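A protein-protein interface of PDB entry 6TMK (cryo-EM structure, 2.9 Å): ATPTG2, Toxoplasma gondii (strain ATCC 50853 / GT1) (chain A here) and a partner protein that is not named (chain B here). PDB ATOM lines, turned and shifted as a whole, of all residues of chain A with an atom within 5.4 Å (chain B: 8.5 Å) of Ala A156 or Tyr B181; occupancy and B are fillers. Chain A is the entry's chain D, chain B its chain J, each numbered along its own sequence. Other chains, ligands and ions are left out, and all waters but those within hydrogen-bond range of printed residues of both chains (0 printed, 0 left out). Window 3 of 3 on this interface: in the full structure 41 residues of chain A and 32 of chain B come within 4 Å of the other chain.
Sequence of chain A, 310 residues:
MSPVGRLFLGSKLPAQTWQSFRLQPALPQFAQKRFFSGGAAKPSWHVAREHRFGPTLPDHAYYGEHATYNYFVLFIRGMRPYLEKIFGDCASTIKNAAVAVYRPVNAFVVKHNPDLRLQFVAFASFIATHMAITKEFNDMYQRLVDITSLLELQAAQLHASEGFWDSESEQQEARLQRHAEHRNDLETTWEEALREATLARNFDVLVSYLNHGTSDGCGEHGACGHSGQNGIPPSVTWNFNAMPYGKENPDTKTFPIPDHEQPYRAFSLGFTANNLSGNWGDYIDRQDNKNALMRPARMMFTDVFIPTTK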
ATOM      1  N   LEU A 151      24.292 -25.537  -8.634  1.00  0.00           N
ATOM      2  CA  LEU A 151      24.677 -25.228 -10.005  1.00  0.00           C
ATOM      3  C   LEU A 151      24.075 -23.911 -10.472  1.00  0.00           C
ATOM      4  O   LEU A 151      24.706 -23.179 -11.242  1.00  0.00           O
ATOM      5  CB  LEU A 151      24.267 -26.366 -10.930  1.00  0.00           C
ATOM      6  CG  LEU A 151      24.980 -27.679 -10.644  1.00  0.00           C
ATOM      7  CD1 LEU A 151      24.386 -28.761 -11.468  1.00  0.00           C
ATOM      8  CD2 LEU A 151      26.452 -27.560 -10.929  1.00  0.00           C
ATOM      9  N   GLU A 152      22.875 -23.582 -10.001  1.00  0.00           N
ATOM     10  CA  GLU A 152      22.328 -22.255 -10.264  1.00  0.00           C
ATOM     11  C   GLU A 152      23.206 -21.169  -9.652  1.00  0.00           C
ATOM     12  O   GLU A 152      23.464 -20.136 -10.282  1.00  0.00           O
ATOM     13  CB  GLU A 152      20.898 -22.166  -9.746  1.00  0.00           C
ATOM     14  CG  GLU A 152      19.905 -22.925 -10.597  1.00  0.00           C
ATOM     15  CD  GLU A 152      18.687 -23.391  -9.822  1.00  0.00           C
ATOM     16  OE1 GLU A 152      18.312 -22.719  -8.840  1.00  0.00           O
ATOM     17  OE2 GLU A 152      18.104 -24.431 -10.195  1.00  0.00           O
ATOM     18  N   LEU A 153      23.653 -21.375  -8.414  1.00  0.00           N
ATOM     19  CA  LEU A 153      24.565 -20.424  -7.786  1.00  0.00           C
ATOM     20  C   LEU A 153      25.866 -20.304  -8.566  1.00  0.00           C
ATOM     21  O   LEU A 153      26.430 -19.212  -8.685  1.00  0.00           O
ATOM     22  CB  LEU A 153      24.851 -20.835  -6.347  1.00  0.00           C
ATOM     23  CG  LEU A 153      23.692 -20.668  -5.376  1.00  0.00           C
ATOM     24  CD1 LEU A 153      23.935 -21.421  -4.086  1.00  0.00           C
ATOM     25  CD2 LEU A 153      23.486 -19.208  -5.100  1.00  0.00           C
ATOM     26  N   GLN A 154      26.372 -21.418  -9.084  1.00  0.00           N
ATOM     27  CA  GLN A 154      27.595 -21.381  -9.874  1.00  0.00           C
ATOM     28  C   GLN A 154      27.388 -20.583 -11.154  1.00  0.00           C
ATOM     29  O   GLN A 154      28.269 -19.823 -11.576  1.00  0.00           O
ATOM     30  CB  GLN A 154      28.029 -22.810 -10.180  1.00  0.00           C
ATOM     31  CG  GLN A 154      29.442 -22.978 -10.641  1.00  0.00           C
ATOM     32  CD  GLN A 154      29.811 -24.432 -10.806  1.00  0.00           C
ATOM     33  OE1 GLN A 154      29.181 -25.310 -10.221  1.00  0.00           O
ATOM     34  NE2 GLN A 154      30.830 -24.699 -11.610  1.00  0.00           N
ATOM     35  N   ALA A 155      26.221 -20.736 -11.780  1.00  0.00           N
ATOM     36  CA  ALA A 155      25.881 -19.930 -12.945  1.00  0.00           C
ATOM     37  C   ALA A 155      25.858 -18.449 -12.599  1.00  0.00           C
ATOM     38  O   ALA A 155      26.381 -17.613 -13.344  1.00  0.00           O
ATOM     39  CB  ALA A 155      24.530 -20.364 -13.499  1.00  0.00           C
ATOM     40  N   ALA A 156      25.224 -18.105 -11.479  1.00  0.00           N
ATOM     41  CA  ALA A 156      25.156 -16.709 -11.064  1.00  0.00           C
ATOM     42  C   ALA A 156      26.533 -16.150 -10.732  1.00  0.00           C
ATOM     43  O   ALA A 156      26.781 -14.957 -10.919  1.00  0.00           O
ATOM     44  CB  ALA A 156      24.226 -16.575  -9.865  1.00  0.00           C
ATOM     45  N   GLN A 157      27.424 -16.993 -10.217  1.00  0.00           N
ATOM     46  CA  GLN A 157      28.790 -16.575  -9.926  1.00  0.00           C
ATOM     47  C   GLN A 157      29.581 -16.349 -11.205  1.00  0.00           C
ATOM     48  O   GLN A 157      30.429 -15.452 -11.270  1.00  0.00           O
ATOM     49  CB  GLN A 157      29.462 -17.628  -9.055  1.00  0.00           C
ATOM     50  CG  GLN A 157      30.701 -17.188  -8.342  1.00  0.00           C
ATOM     51  CD  GLN A 157      31.475 -18.358  -7.793  1.00  0.00           C
ATOM     52  OE1 GLN A 157      31.828 -19.280  -8.525  1.00  0.00           O
ATOM     53  NE2 GLN A 157      31.716 -18.346  -6.493  1.00  0.00           N
ATOM     54  N   LEU A 158      29.322 -17.161 -12.227  1.00  0.00           N
ATOM     55  CA  LEU A 158      29.934 -16.941 -13.531  1.00  0.00           C
ATOM     56  C   LEU A 158      29.533 -15.586 -14.099  1.00  0.00           C
ATOM     57  O   LEU A 158      30.377 -14.836 -14.602  1.00  0.00           O
ATOM     58  CB  LEU A 158      29.544 -18.072 -14.471  1.00  0.00           C
ATOM     59  CG  LEU A 158      30.241 -18.153 -15.817  1.00  0.00           C
ATOM     60  CD1 LEU A 158      31.658 -18.645 -15.653  1.00  0.00           C
ATOM     61  CD2 LEU A 158      29.459 -19.087 -16.685  1.00  0.00           C
ATOM     62  N   HIS A 159      28.242 -15.262 -14.043  1.00  0.00           N
ATOM     63  CA  HIS A 159      27.782 -13.960 -14.508  1.00  0.00           C
ATOM     64  C   HIS A 159      28.465 -12.822 -13.770  1.00  0.00           C
ATOM     65  O   HIS A 159      28.730 -11.771 -14.361  1.00  0.00           O
ATOM     66  CB  HIS A 159      26.275 -13.834 -14.327  1.00  0.00           C
ATOM     67  CG  HIS A 159      25.471 -14.415 -15.440  1.00  0.00           C
ATOM     68  ND1 HIS A 159      24.305 -15.114 -15.223  1.00  0.00           N
ATOM     69  CD2 HIS A 159      25.641 -14.370 -16.781  1.00  0.00           C
ATOM     70  CE1 HIS A 159      23.801 -15.492 -16.383  1.00  0.00           C
ATOM     71  NE2 HIS A 159      24.592 -15.051 -17.344  1.00  0.00           N
ATOM     72  N   ALA A 160      28.758 -13.006 -12.484  1.00  0.00           N
ATOM     73  CA  ALA A 160      29.384 -11.942 -11.716  1.00  0.00           C
ATOM     74  C   ALA A 160      30.841 -11.753 -12.108  1.00  0.00           C
ATOM     75  O   ALA A 160      31.359 -10.634 -12.035  1.00  0.00           O
ATOM     76  CB  ALA A 160      29.266 -12.249 -10.230  1.00  0.00           C
ATOM     77  N   TRP A 165      26.034  -8.554 -13.310  1.00  0.00           N
ATOM     78  CA  TRP A 165      25.242  -7.925 -12.269  1.00  0.00           C
ATOM     79  C   TRP A 165      25.671  -6.494 -11.993  1.00  0.00           C
ATOM     80  O   TRP A 165      24.939  -5.766 -11.316  1.00  0.00           O
ATOM     81  CB  TRP A 165      25.336  -8.733 -10.980  1.00  0.00           C
ATOM     82  CG  TRP A 165      25.005 -10.178 -11.113  1.00  0.00           C
ATOM     83  CD1 TRP A 165      25.742 -11.218 -10.657  1.00  0.00           C
ATOM     84  CD2 TRP A 165      23.846 -10.749 -11.725  1.00  0.00           C
ATOM     85  NE1 TRP A 165      25.129 -12.402 -10.950  1.00  0.00           N
ATOM     86  CE2 TRP A 165      23.960 -12.141 -11.606  1.00  0.00           C
ATOM     87  CE3 TRP A 165      22.725 -10.221 -12.359  1.00  0.00           C
ATOM     88  CZ2 TRP A 165      23.000 -13.007 -12.099  1.00  0.00           C
ATOM     89  CZ3 TRP A 165      21.782 -11.085 -12.848  1.00  0.00           C
ATOM     90  CH2 TRP A 165      21.924 -12.460 -12.715  1.00  0.00           C
ATOM     91  N   ARG B 142      13.786 -19.771  -0.627  1.00  0.00           N
ATOM     92  CA  ARG B 142      13.043 -18.785  -1.408  1.00  0.00           C
ATOM     93  C   ARG B 142      12.632 -19.431  -2.721  1.00  0.00           C
ATOM     94  O   ARG B 142      13.459 -19.552  -3.640  1.00  0.00           O
ATOM     95  CB  ARG B 142      13.875 -17.537  -1.653  1.00  0.00           C
ATOM     96  CG  ARG B 142      14.132 -16.721  -0.421  1.00  0.00           C
ATOM     97  CD  ARG B 142      14.982 -15.523  -0.723  1.00  0.00           C
ATOM     98  NE  ARG B 142      14.315 -14.565  -1.591  1.00  0.00           N
ATOM     99  CZ  ARG B 142      13.426 -13.671  -1.182  1.00  0.00           C
ATOM    100  NH1 ARG B 142      12.881 -12.847  -2.050  1.00  0.00           N
ATOM    101  NH2 ARG B 142      13.080 -13.600   0.086  1.00  0.00           N
ATOM    102  N   LEU B 145      12.469 -18.871  -7.658  1.00  0.00           N
ATOM    103  CA  LEU B 145      13.190 -19.384  -8.813  1.00  0.00           C
ATOM    104  C   LEU B 145      12.643 -20.735  -9.257  1.00  0.00           C
ATOM    105  O   LEU B 145      12.446 -20.976 -10.456  1.00  0.00           O
ATOM    106  CB  LEU B 145      14.669 -19.490  -8.464  1.00  0.00           C
ATOM    107  CG  LEU B 145      15.682 -19.744  -9.567  1.00  0.00           C
ATOM    108  CD1 LEU B 145      15.605 -18.667 -10.599  1.00  0.00           C
ATOM    109  CD2 LEU B 145      17.046 -19.798  -8.973  1.00  0.00           C
ATOM    110  N   LEU B 174      16.184 -13.863 -14.095  1.00  0.00           N
ATOM    111  CA  LEU B 174      17.533 -13.427 -13.757  1.00  0.00           C
ATOM    112  C   LEU B 174      17.550 -12.609 -12.474  1.00  0.00           C
ATOM    113  O   LEU B 174      18.518 -12.674 -11.712  1.00  0.00           O
ATOM    114  CB  LEU B 174      18.145 -12.644 -14.910  1.00  0.00           C
ATOM    115  CG  LEU B 174      18.414 -13.486 -16.151  1.00  0.00           C
ATOM    116  CD1 LEU B 174      18.646 -12.619 -17.353  1.00  0.00           C
ATOM    117  CD2 LEU B 174      19.582 -14.405 -15.913  1.00  0.00           C
ATOM    118  N   PHE B 175      16.493 -11.843 -12.222  1.00  0.00           N
ATOM    119  CA  PHE B 175      16.354 -11.131 -10.962  1.00  0.00           C
ATOM    120  C   PHE B 175      16.348 -12.095  -9.786  1.00  0.00           C
ATOM    121  O   PHE B 175      17.027 -11.871  -8.777  1.00  0.00           O
ATOM    122  CB  PHE B 175      15.068 -10.314 -10.998  1.00  0.00           C
ATOM    123  CG  PHE B 175      14.909  -9.374  -9.856  1.00  0.00           C
ATOM    124  CD1 PHE B 175      15.392  -8.094  -9.932  1.00  0.00           C
ATOM    125  CD2 PHE B 175      14.265  -9.769  -8.707  1.00  0.00           C
ATOM    126  CE1 PHE B 175      15.246  -7.233  -8.891  1.00  0.00           C
ATOM    127  CE2 PHE B 175      14.120  -8.910  -7.663  1.00  0.00           C
ATOM    128  CZ  PHE B 175      14.611  -7.640  -7.754  1.00  0.00           C
ATOM    129  N   LYS B 176      15.588 -13.181  -9.900  1.00  0.00           N
ATOM    130  CA  LYS B 176      15.528 -14.141  -8.807  1.00  0.00           C
ATOM    131  C   LYS B 176      16.857 -14.872  -8.643  1.00  0.00           C
ATOM    132  O   LYS B 176      17.270 -15.178  -7.518  1.00  0.00           O
ATOM    133  CB  LYS B 176      14.382 -15.117  -9.045  1.00  0.00           C
ATOM    134  CG  LYS B 176      13.038 -14.477  -8.908  1.00  0.00           C
ATOM    135  CD  LYS B 176      11.941 -15.284  -9.517  1.00  0.00           C
ATOM    136  CE  LYS B 176      10.623 -14.699  -9.130  1.00  0.00           C
ATOM    137  NZ  LYS B 176       9.528 -15.184  -9.977  1.00  0.00           N
ATOM    138  N   LEU B 177      17.533 -15.164  -9.753  1.00  0.00           N
ATOM    139  CA  LEU B 177      18.871 -15.745  -9.689  1.00  0.00           C
ATOM    140  C   LEU B 177      19.839 -14.831  -8.941  1.00  0.00           C
ATOM    141  O   LEU B 177      20.603 -15.280  -8.076  1.00  0.00           O
ATOM    142  CB  LEU B 177      19.358 -16.011 -11.108  1.00  0.00           C
ATOM    143  CG  LEU B 177      20.556 -16.910 -11.365  1.00  0.00           C
ATOM    144  CD1 LEU B 177      20.238 -18.350 -11.102  1.00  0.00           C
ATOM    145  CD2 LEU B 177      20.989 -16.719 -12.785  1.00  0.00           C
ATOM    146  N   ARG B 178      19.831 -13.542  -9.280  1.00  0.00           N
ATOM    147  CA  ARG B 178      20.663 -12.569  -8.582  1.00  0.00           C
ATOM    148  C   ARG B 178      20.338 -12.513  -7.096  1.00  0.00           C
ATOM    149  O   ARG B 178      21.243 -12.416  -6.259  1.00  0.00           O
ATOM    150  CB  ARG B 178      20.482 -11.200  -9.223  1.00  0.00           C
ATOM    151  CG  ARG B 178      21.355 -10.111  -8.658  1.00  0.00           C
ATOM    152  CD  ARG B 178      21.101  -8.797  -9.341  1.00  0.00           C
ATOM    153  NE  ARG B 178      21.681  -7.682  -8.606  1.00  0.00           N
ATOM    154  CZ  ARG B 178      21.055  -6.998  -7.657  1.00  0.00           C
ATOM    155  NH1 ARG B 178      19.821  -7.302  -7.303  1.00  0.00           N
ATOM    156  NH2 ARG B 178      21.675  -6.011  -7.052  1.00  0.00           N
ATOM    157  N   GLU B 179      19.051 -12.535  -6.750  1.00  0.00           N
ATOM    158  CA  GLU B 179      18.674 -12.488  -5.342  1.00  0.00           C
ATOM    159  C   GLU B 179      19.179 -13.713  -4.599  1.00  0.00           C
ATOM    160  O   GLU B 179      19.652 -13.605  -3.464  1.00  0.00           O
ATOM    161  CB  GLU B 179      17.161 -12.357  -5.189  1.00  0.00           C
ATOM    162  CG  GLU B 179      16.643 -10.962  -5.394  1.00  0.00           C
ATOM    163  CD  GLU B 179      15.213 -10.790  -4.903  1.00  0.00           C
ATOM    164  OE1 GLU B 179      14.897  -9.734  -4.316  1.00  0.00           O
ATOM    165  OE2 GLU B 179      14.401 -11.715  -5.101  1.00  0.00           O
ATOM    166  N   GLN B 180      19.083 -14.887  -5.219  1.00  0.00           N
ATOM    167  CA  GLN B 180      19.630 -16.094  -4.614  1.00  0.00           C
ATOM    168  C   GLN B 180      21.129 -15.953  -4.378  1.00  0.00           C
ATOM    169  O   GLN B 180      21.641 -16.283  -3.298  1.00  0.00           O
ATOM    170  CB  GLN B 180      19.334 -17.285  -5.523  1.00  0.00           C
ATOM    171  CG  GLN B 180      19.603 -18.637  -4.931  1.00  0.00           C
ATOM    172  CD  GLN B 180      19.523 -19.743  -5.962  1.00  0.00           C
ATOM    173  OE1 GLN B 180      19.376 -19.483  -7.155  1.00  0.00           O
ATOM    174  NE2 GLN B 180      19.635 -20.984  -5.511  1.00  0.00           N
ATOM    175  N   TYR B 181      21.851 -15.462  -5.389  1.00  0.00           N
ATOM    176  CA  TYR B 181      23.289 -15.274  -5.254  1.00  0.00           C
ATOM    177  C   TYR B 181      23.620 -14.345  -4.095  1.00  0.00           C
ATOM    178  O   TYR B 181      24.489 -14.648  -3.271  1.00  0.00           O
ATOM    179  CB  TYR B 181      23.864 -14.719  -6.553  1.00  0.00           C
ATOM    180  CG  TYR B 181      25.342 -14.432  -6.499  1.00  0.00           C
ATOM    181  CD1 TYR B 181      26.263 -15.447  -6.315  1.00  0.00           C
ATOM    182  CD2 TYR B 181      25.816 -13.138  -6.625  1.00  0.00           C
ATOM    183  CE1 TYR B 181      27.607 -15.181  -6.263  1.00  0.00           C
ATOM    184  CE2 TYR B 181      27.158 -12.865  -6.571  1.00  0.00           C
ATOM    185  CZ  TYR B 181      28.051 -13.887  -6.387  1.00  0.00           C
ATOM    186  OH  TYR B 181      29.396 -13.605  -6.334  1.00  0.00           O
ATOM    187  N   LEU B 182      22.928 -13.211  -4.011  1.00  0.00           N
ATOM    188  CA  LEU B 182      23.198 -12.258  -2.943  1.00  0.00           C
ATOM    189  C   LEU B 182      22.851 -12.831  -1.579  1.00  0.00           C
ATOM    190  O   LEU B 182      23.569 -12.595  -0.601  1.00  0.00           O
ATOM    191  CB  LEU B 182      22.420 -10.973  -3.186  1.00  0.00           C
ATOM    192  CG  LEU B 182      22.826 -10.149  -4.392  1.00  0.00           C
ATOM    193  CD1 LEU B 182      21.941  -8.955  -4.483  1.00  0.00           C
ATOM    194  CD2 LEU B 182      24.271  -9.725  -4.296  1.00  0.00           C
ATOM    195  N   VAL B 183      21.742 -13.558  -1.484  1.00  0.00           N
ATOM    196  CA  VAL B 183      21.324 -14.100  -0.200  1.00  0.00           C
ATOM    197  C   VAL B 183      22.331 -15.121   0.304  1.00  0.00           C
ATOM    198  O   VAL B 183      22.580 -15.222   1.511  1.00  0.00           O
ATOM    199  CB  VAL B 183      19.913 -14.700  -0.316  1.00  0.00           C
ATOM    200  CG1 VAL B 183      19.627 -15.598   0.839  1.00  0.00           C
ATOM    201  CG2 VAL B 183      18.887 -13.609  -0.385  1.00  0.00           C
ATOM    202  N   ASN B 184      22.928 -15.889  -0.603  1.00  0.00           N
ATOM    203  CA  ASN B 184      23.943 -16.847  -0.188  1.00  0.00           C
ATOM    204  C   ASN B 184      25.319 -16.218  -0.009  1.00  0.00           C
ATOM    205  O   ASN B 184      26.154 -16.784   0.701  1.00  0.00           O
ATOM    206  CB  ASN B 184      24.001 -18.005  -1.174  1.00  0.00           C
ATOM    207  CG  ASN B 184      22.909 -19.013  -0.931  1.00  0.00           C
ATOM    208  OD1 ASN B 184      23.081 -19.956  -0.166  1.00  0.00           O
ATOM    209  ND2 ASN B 184      21.769 -18.809  -1.561  1.00  0.00           N
ATOM    210  N   LYS B 185      25.565 -15.064  -0.623  1.00  0.00           N
ATOM    211  CA  LYS B 185      26.860 -14.409  -0.513  1.00  0.00           C
ATOM    212  C   LYS B 185      26.952 -13.581   0.760  1.00  0.00           C
ATOM    213  O   LYS B 185      27.904 -13.720   1.535  1.00  0.00           O
ATOM    214  CB  LYS B 185      27.091 -13.525  -1.732  1.00  0.00           C
ATOM    215  CG  LYS B 185      28.511 -13.125  -1.943  1.00  0.00           C
ATOM    216  CD  LYS B 185      28.623 -12.137  -3.069  1.00  0.00           C
ATOM    217  CE  LYS B 185      29.891 -11.341  -2.978  1.00  0.00           C
ATOM    218  NZ  LYS B 185      31.035 -12.233  -2.719  1.00  0.00           N
ATOM    219  N   TYR B 186      25.986 -12.700   0.982  1.00  0.00           N
ATOM    220  CA  TYR B 186      25.958 -11.846   2.156  1.00  0.00           C
ATOM    221  C   TYR B 186      24.976 -12.423   3.163  1.00  0.00           C
ATOM    222  O   TYR B 186      23.788 -12.575   2.864  1.00  0.00           O
ATOM    223  CB  TYR B 186      25.565 -10.421   1.787  1.00  0.00           C
ATOM    224  CG  TYR B 186      26.433  -9.792   0.734  1.00  0.00           C
ATOM    225  CD1 TYR B 186      27.666  -9.263   1.056  1.00  0.00           C
ATOM    226  CD2 TYR B 186      26.012  -9.708  -0.579  1.00  0.00           C
ATOM    227  CE1 TYR B 186      28.457  -8.685   0.105  1.00  0.00           C
ATOM    228  CE2 TYR B 186      26.796  -9.129  -1.536  1.00  0.00           C
ATOM    229  CZ  TYR B 186      28.017  -8.613  -1.192  1.00  0.00           C
ATOM    230  OH  TYR B 186      28.807  -8.033  -2.153  1.00  0.00           O
ATOM    231  N   GLU B 187      25.471 -12.734   4.353  1.00  0.00           N
ATOM    232  CA  GLU B 187      24.632 -13.295   5.397  1.00  0.00           C
ATOM    233  C   GLU B 187      23.791 -12.198   6.030  1.00  0.00           C
ATOM    234  O   GLU B 187      24.322 -11.186   6.498  1.00  0.00           O
ATOM    235  CB  GLU B 187      25.498 -13.965   6.458  1.00  0.00           C
ATOM    236  CG  GLU B 187      24.820 -15.078   7.219  1.00  0.00           C
ATOM    237  CD  GLU B 187      25.743 -15.745   8.213  1.00  0.00           C
ATOM    238  OE1 GLU B 187      26.926 -15.354   8.281  1.00  0.00           O
ATOM    239  OE2 GLU B 187      25.286 -16.657   8.932  1.00  0.00           O
ATOM    240  N   ILE B 189      21.367 -10.346   4.526  1.00  0.00           N
ATOM    241  CA  ILE B 189      20.902  -9.262   3.679  1.00  0.00           C
ATOM    242  C   ILE B 189      19.377  -9.215   3.676  1.00  0.00           C
ATOM    243  O   ILE B 189      18.696 -10.235   3.831  1.00  0.00           O
ATOM    244  CB  ILE B 189      21.485  -9.438   2.266  1.00  0.00           C
ATOM    245  CG1 ILE B 189      21.293  -8.184   1.421  1.00  0.00           C
ATOM    246  CG2 ILE B 189      20.908 -10.661   1.594  1.00  0.00           C
ATOM    247  CD1 ILE B 189      22.077  -8.214   0.170  1.00  0.00           C
ATOM    248  N   VAL B 194      17.460  -6.916  -1.309  1.00  0.00           N
ATOM    249  CA  VAL B 194      16.702  -8.080  -1.752  1.00  0.00           C
ATOM    250  C   VAL B 194      15.355  -8.054  -1.054  1.00  0.00           C
ATOM    251  O   VAL B 194      15.244  -7.631   0.096  1.00  0.00           O
ATOM    252  CB  VAL B 194      17.407  -9.417  -1.435  1.00  0.00           C
ATOM    253  CG1 VAL B 194      18.789  -9.458  -1.992  1.00  0.00           C
ATOM    254  CG2 VAL B 194      17.449  -9.629   0.061  1.00  0.00           C
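Of the printed residues of chain B, Ala A156 touches Leu B177 and Tyr B181.
Of the printed residues of chain A, Gln B180 touches Glu A152 and Leu A153.
Of the printed residues of chain A, Leu B174 touches Trp A165 (3.6 Å).
The nearest printed residue of chain B that does not touch Leu A153 is Leu B177 (5.3 Å).
Of the 11 printed residues of chain A, 4 touch a printed residue of chain B.
Hydrophobic or aromatic side chains of chain A within 4 Å of the printed part of chain B: Leu A153, Ala A156 and Trp A165.
Among the printed residues, 10 pairs touch across the chains.
Among the printed residues, no Asp or Glu carboxylate lies within 4 Å of a Lys or Arg side-chain nitrogen of the other chain.
Among the printed residues, merely in contact across the chains: Glu A152 with Leu B145 (3.2 Å), Glu A152 with Leu B177 (3.8 Å), Glu A152 with Gln B180 (3.8 Å), Leu A153 with Gln B180 (3.9 Å), Leu A153 with Tyr B181 (3.9 Å), Leu A153 with Asn B184 (3.95 Å), Ala A156 with Leu B177 (3.98 Å), Ala A156 with Tyr B181 (3.8 Å), Trp A165 with Leu B174 (3.6 Å) and Trp A165 with Arg B178 (3.7 Å).
The backbone carbonyl oxygen of Ala A156 is in hydrogen-bond range of the indole nitrogen of Trp A165.
The backbone carbonyl oxygen (O) of Gln B180 sits at hydrogen-bond distance from the side-chain amide nitrogen (ND2) of Asn B184 (3.1 Å).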
